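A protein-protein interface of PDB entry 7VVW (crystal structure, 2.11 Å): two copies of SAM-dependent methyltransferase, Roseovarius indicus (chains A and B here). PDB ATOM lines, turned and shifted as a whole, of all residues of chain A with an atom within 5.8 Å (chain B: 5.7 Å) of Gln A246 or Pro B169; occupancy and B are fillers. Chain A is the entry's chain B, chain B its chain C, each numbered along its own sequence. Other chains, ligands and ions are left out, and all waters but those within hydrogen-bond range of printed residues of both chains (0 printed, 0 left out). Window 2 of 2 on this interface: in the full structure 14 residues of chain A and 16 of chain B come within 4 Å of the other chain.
The backbone carbonyl oxygen of Tyr B168 is in hydrogen-bond range of the side-chain amide nitrogen of Gln A246 (3.3 Å). OE1 of Gln A246 lies close to O of Pro B169, 3.4 Å away. NE2 of Gln A246 sits at hydrogen-bond distance from O of Asp B166 (2.6 Å). The guanidinium group (NE) of Arg A251 lies within salt-bridge range of the side-chain carboxylate (OD2) of Asp B166 (3.9 Å). N of Ser B172 sits close to OE1 of Gln A246, 3.3 Å away.
Among the printed residues, pairs that only touch across the chains: Pro A169 with Ser B167, Pro A169 with Pro B169, Ala A245 with Asp B166, Gln A246 with Ser B167, Gln A246 with Asn B171, Thr A247 with Asn B171 and Thr A247 with Ser B172.
Of the printed residues of chain B, Gln A246 touches Asp B166 (2.6 Å), Ser B167 (3.9 Å), Tyr B168 (3.3 Å), Pro B169 (3.4 Å), Asn B171 (3.99 Å) and Ser B172 (3.2 Å). Printed residues of chain B within 4 Å of Thr A247: Asn B171 and Ser B172. Of the printed residues of chain A, Asp B166 touches Ala A245, Gln A246 and Arg A251. Pro B169 touches just these residues of chain A: Pro A169 (3.9 Å) and Gln A246 (3.4 Å). The nearest printed residue of chain B that does not touch Gln A246 is Phe B170 (5.2 Å). The nearest printed residue of chain A that does not touch Pro B169 is Thr A247 (8.3 Å). The nearest printed residue of chain B that does not touch Ala A245 is Asn B171 (5.3 Å).
Pro A169 touches its own counterpart, Pro B169. 1 position is printed for both chains. Of the 12 pairs that touch across the chains among the printed residues, 1 has its exchanged pair printed and touching as well.
OD1 of Asp B166 sits close to OD1 of Asn B171, at 3.1 Å. O of Pro B169 lies within hydrogen-bond range of OG of Ser B172 (3.0 Å).
Of the 10 printed residues of chain B, 6 touch a printed residue of chain A. Hydrophobic or aromatic side chains of chain B within 4 Å of the printed part of chain A: Pro B169. Printed residues of chain A that touch a printed residue of chain B: Pro A169, Ala A245, Gln A246, Thr A247 and Arg A251. Hydrophobic or aromatic side chains of chain A that line the printed part of chain B: Pro A169 and Ala A245. Among the printed residues, Asp or Glu carboxylates within 4 Å of a Lys or Arg side-chain nitrogen of the other chain: Arg A251 with Asp B166.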
ATOM      1  N   PRO A 169       7.046 -22.915  19.576  1.00  0.00           N
ATOM      2  CA  PRO A 169       8.145 -23.430  20.401  1.00  0.00           C
ATOM      3  C   PRO A 169       8.921 -24.557  19.736  1.00  0.00           C
ATOM      4  O   PRO A 169      10.147 -24.597  19.867  1.00  0.00           O
ATOM      5  CB  PRO A 169       7.425 -23.901  21.670  1.00  0.00           C
ATOM      6  CG  PRO A 169       6.194 -22.980  21.751  1.00  0.00           C
ATOM      7  CD  PRO A 169       5.770 -22.827  20.314  1.00  0.00           C
ATOM      8  N   LEU A 244      23.644 -22.973  23.085  1.00  0.00           N
ATOM      9  CA  LEU A 244      23.390 -22.778  24.496  1.00  0.00           C
ATOM     10  C   LEU A 244      21.884 -22.938  24.631  1.00  0.00           C
ATOM     11  O   LEU A 244      21.130 -22.595  23.720  1.00  0.00           O
ATOM     12  CB  LEU A 244      23.822 -21.382  24.938  1.00  0.00           C
ATOM     13  CG  LEU A 244      25.099 -21.302  25.778  1.00  0.00           C
ATOM     14  CD1 LEU A 244      26.324 -21.590  24.922  1.00  0.00           C
ATOM     15  CD2 LEU A 244      25.218 -19.942  26.449  1.00  0.00           C
ATOM     16  N   ALA A 245      21.455 -23.465  25.740  1.00  0.00           N
ATOM     17  CA  ALA A 245      20.066 -23.699  25.972  1.00  0.00           C
ATOM     18  C   ALA A 245      19.277 -22.403  26.025  1.00  0.00           C
ATOM     19  O   ALA A 245      19.856 -21.369  26.218  1.00  0.00           O
ATOM     20  CB  ALA A 245      19.946 -24.446  27.259  1.00  0.00           C
ATOM     21  N   GLN A 246      17.964 -22.450  25.861  1.00  0.00           N
ATOM     22  CA  GLN A 246      17.175 -21.238  25.880  1.00  0.00           C
ATOM     23  C   GLN A 246      17.421 -20.407  27.109  1.00  0.00           C
ATOM     24  O   GLN A 246      17.287 -19.215  27.103  1.00  0.00           O
ATOM     25  CB  GLN A 246      15.687 -21.590  25.820  1.00  0.00           C
ATOM     26  CG  GLN A 246      14.724 -20.490  26.183  1.00  0.00           C
ATOM     27  CD  GLN A 246      13.282 -20.791  25.800  1.00  0.00           C
ATOM     28  OE1 GLN A 246      12.405 -19.979  25.974  1.00  0.00           O
ATOM     29  NE2 GLN A 246      13.049 -21.940  25.259  1.00  0.00           N
ATOM     30  N   THR A 247      17.768 -21.087  28.184  1.00  0.00           N
ATOM     31  CA  THR A 247      17.934 -20.433  29.451  1.00  0.00           C
ATOM     32  C   THR A 247      18.667 -19.102  29.413  1.00  0.00           C
ATOM     33  O   THR A 247      17.990 -18.104  29.583  1.00  0.00           O
ATOM     34  CB  THR A 247      18.380 -21.382  30.569  1.00  0.00           C
ATOM     35  OG1 THR A 247      19.736 -21.756  30.386  1.00  0.00           O
ATOM     36  CG2 THR A 247      17.514 -22.610  30.576  1.00  0.00           C
ATOM     37  N   GLY A 248      20.000 -19.060  29.206  1.00  0.00           N
ATOM     38  CA  GLY A 248      20.886 -20.207  29.003  1.00  0.00           C
ATOM     39  C   GLY A 248      22.359 -19.920  28.706  1.00  0.00           C
ATOM     40  O   GLY A 248      22.611 -18.995  28.019  1.00  0.00           O
ATOM     41  N   ARG A 251      24.029 -26.802  27.661  1.00  0.00           N
ATOM     42  CA  ARG A 251      23.133 -27.703  27.041  1.00  0.00           C
ATOM     43  C   ARG A 251      23.918 -28.795  26.336  1.00  0.00           C
ATOM     44  O   ARG A 251      24.657 -28.544  25.431  1.00  0.00           O
ATOM     45  CB  ARG A 251      22.272 -26.916  26.038  1.00  0.00           C
ATOM     46  CG  ARG A 251      21.467 -27.741  25.059  1.00  0.00           C
ATOM     47  CD  ARG A 251      20.253 -27.034  24.469  1.00  0.00           C
ATOM     48  NE  ARG A 251      19.454 -27.905  23.598  1.00  0.00           N
ATOM     49  CZ  ARG A 251      19.575 -28.021  22.269  1.00  0.00           C
ATOM     50  NH1 ARG A 251      20.433 -27.293  21.601  1.00  0.00           N
ATOM     51  NH2 ARG A 251      18.812 -28.871  21.595  1.00  0.00           N
ATOM     52  N   ASP B 166      13.476 -27.918  26.362  1.00  0.00           N
ATOM     53  CA  ASP B 166      14.144 -26.655  26.085  1.00  0.00           C
ATOM     54  C   ASP B 166      13.306 -25.715  25.236  1.00  0.00           C
ATOM     55  O   ASP B 166      13.578 -24.516  25.228  1.00  0.00           O
ATOM     56  CB  ASP B 166      15.485 -26.910  25.388  1.00  0.00           C
ATOM     57  CG  ASP B 166      16.269 -25.629  25.128  1.00  0.00           C
ATOM     58  OD1 ASP B 166      16.620 -24.937  26.103  1.00  0.00           O
ATOM     59  OD2 ASP B 166      16.519 -25.307  23.946  1.00  0.00           O
ATOM     60  N   SER B 167      12.318 -26.232  24.500  1.00  0.00           N
ATOM     61  CA  SER B 167      11.530 -25.388  23.624  1.00  0.00           C
ATOM     62  C   SER B 167      10.428 -24.645  24.366  1.00  0.00           C
ATOM     63  O   SER B 167       9.833 -23.733  23.791  1.00  0.00           O
ATOM     64  CB  SER B 167      10.907 -26.220  22.490  1.00  0.00           C
ATOM     65  OG  SER B 167       9.704 -26.885  22.889  1.00  0.00           O
ATOM     66  N   TYR B 168      10.158 -24.993  25.614  1.00  0.00           N
ATOM     67  CA  TYR B 168       9.000 -24.443  26.295  1.00  0.00           C
ATOM     68  C   TYR B 168       9.169 -22.949  26.527  1.00  0.00           C
ATOM     69  O   TYR B 168      10.244 -22.511  26.960  1.00  0.00           O
ATOM     70  CB  TYR B 168       8.777 -25.157  27.617  1.00  0.00           C
ATOM     71  CG  TYR B 168       8.019 -26.431  27.436  1.00  0.00           C
ATOM     72  CD1 TYR B 168       6.638 -26.415  27.327  1.00  0.00           C
ATOM     73  CD2 TYR B 168       8.682 -27.646  27.308  1.00  0.00           C
ATOM     74  CE1 TYR B 168       5.927 -27.578  27.141  1.00  0.00           C
ATOM     75  CE2 TYR B 168       7.976 -28.822  27.110  1.00  0.00           C
ATOM     76  CZ  TYR B 168       6.592 -28.770  27.037  1.00  0.00           C
ATOM     77  OH  TYR B 168       5.856 -29.902  26.859  1.00  0.00           O
ATOM     78  N   PRO B 169       8.141 -22.134  26.236  1.00  0.00           N
ATOM     79  CA  PRO B 169       8.197 -20.692  26.538  1.00  0.00           C
ATOM     80  C   PRO B 169       8.787 -20.375  27.900  1.00  0.00           C
ATOM     81  O   PRO B 169       9.666 -19.520  28.003  1.00  0.00           O
ATOM     82  CB  PRO B 169       6.728 -20.272  26.462  1.00  0.00           C
ATOM     83  CG  PRO B 169       6.165 -21.192  25.348  1.00  0.00           C
ATOM     84  CD  PRO B 169       6.911 -22.513  25.513  1.00  0.00           C
ATOM     85  N   PHE B 170       8.339 -21.065  28.945  1.00  0.00           N
ATOM     86  CA  PHE B 170       8.824 -20.732  30.276  1.00  0.00           C
ATOM     87  C   PHE B 170      10.148 -21.405  30.616  1.00  0.00           C
ATOM     88  O   PHE B 170      10.642 -21.231  31.735  1.00  0.00           O
ATOM     89  CB  PHE B 170       7.755 -21.073  31.316  1.00  0.00           C
ATOM     90  CG  PHE B 170       6.638 -20.076  31.344  1.00  0.00           C
ATOM     91  CD1 PHE B 170       5.554 -20.214  30.494  1.00  0.00           C
ATOM     92  CD2 PHE B 170       6.706 -18.953  32.177  1.00  0.00           C
ATOM     93  CE1 PHE B 170       4.515 -19.267  30.505  1.00  0.00           C
ATOM     94  CE2 PHE B 170       5.698 -18.025  32.199  1.00  0.00           C
ATOM     95  CZ  PHE B 170       4.589 -18.170  31.354  1.00  0.00           C
ATOM     96  N   ASN B 171      10.746 -22.145  29.682  1.00  0.00           N
ATOM     97  CA  ASN B 171      12.124 -22.551  29.911  1.00  0.00           C
ATOM     98  C   ASN B 171      13.064 -21.351  29.922  1.00  0.00           C
ATOM     99  O   ASN B 171      14.123 -21.415  30.542  1.00  0.00           O
ATOM    100  CB  ASN B 171      12.582 -23.565  28.868  1.00  0.00           C
ATOM    101  CG  ASN B 171      13.825 -24.299  29.316  1.00  0.00           C
ATOM    102  OD1 ASN B 171      14.823 -24.362  28.599  1.00  0.00           O
ATOM    103  ND2 ASN B 171      13.779 -24.833  30.536  1.00  0.00           N
ATOM    104  N   SER B 172      12.690 -20.254  29.256  1.00  0.00           N
ATOM    105  CA  SER B 172      13.485 -19.028  29.307  1.00  0.00           C
ATOM    106  C   SER B 172      13.669 -18.493  30.729  1.00  0.00           C
ATOM    107  O   SER B 172      14.592 -17.703  30.965  1.00  0.00           O
ATOM    108  CB  SER B 172      12.837 -17.964  28.436  1.00  0.00           C
ATOM    109  OG  SER B 172      11.652 -17.500  29.059  1.00  0.00           O
ATOM    110  N   VAL B 173      12.820 -18.882  31.676  1.00  0.00           N
ATOM    111  CA  VAL B 173      13.023 -18.553  33.078  1.00  0.00           C
ATOM    112  C   VAL B 173      13.281 -19.809  33.916  1.00  0.00           C
ATOM    113  O   VAL B 173      13.086 -19.796  35.127  1.00  0.00           O
ATOM    114  CB  VAL B 173      11.857 -17.719  33.639  1.00  0.00           C
ATOM    115  CG1 VAL B 173      11.737 -16.388  32.874  1.00  0.00           C
ATOM    116  CG2 VAL B 173      10.553 -18.480  33.573  1.00  0.00           C
ATOM    117  N   GLU B 179       6.318 -26.394  33.091  1.00  0.00           N
ATOM    118  CA  GLU B 179       5.345 -26.136  32.037  1.00  0.00           C
ATOM    119  C   GLU B 179       4.996 -27.421  31.303  1.00  0.00           C
ATOM    120  O   GLU B 179       3.839 -27.628  30.920  1.00  0.00           O
ATOM    121  CB  GLU B 179       5.859 -25.092  31.042  1.00  0.00           C
ATOM    122  CG  GLU B 179       4.752 -24.705  30.044  1.00  0.00           C
ATOM    123  CD  GLU B 179       5.083 -23.518  29.154  1.00  0.00           C
ATOM    124  OE1 GLU B 179       6.271 -23.189  29.029  1.00  0.00           O
ATOM    125  OE2 GLU B 179       4.141 -22.916  28.568  1.00  0.00           O
ATOM    126  N   ARG B 183       1.103 -28.958  30.628  1.00  0.00           N
ATOM    127  CA  ARG B 183       0.559 -29.434  29.357  1.00  0.00           C
ATOM    128  C   ARG B 183      -0.064 -30.814  29.496  1.00  0.00           C
ATOM    129  O   ARG B 183      -1.042 -31.133  28.806  1.00  0.00           O
ATOM    130  CB  ARG B 183       1.661 -29.494  28.296  1.00  0.00           C
ATOM    131  CG  ARG B 183       2.406 -28.214  28.062  1.00  0.00           C
ATOM    132  CD  ARG B 183       1.474 -27.109  27.510  1.00  0.00           C
ATOM    133  NE  ARG B 183       2.243 -25.883  27.341  1.00  0.00           N
ATOM    134  CZ  ARG B 183       2.792 -25.504  26.189  1.00  0.00           C
ATOM    135  NH1 ARG B 183       2.651 -26.248  25.105  1.00  0.00           N
ATOM    136  NH2 ARG B 183       3.480 -24.378  26.122  1.00  0.00           N
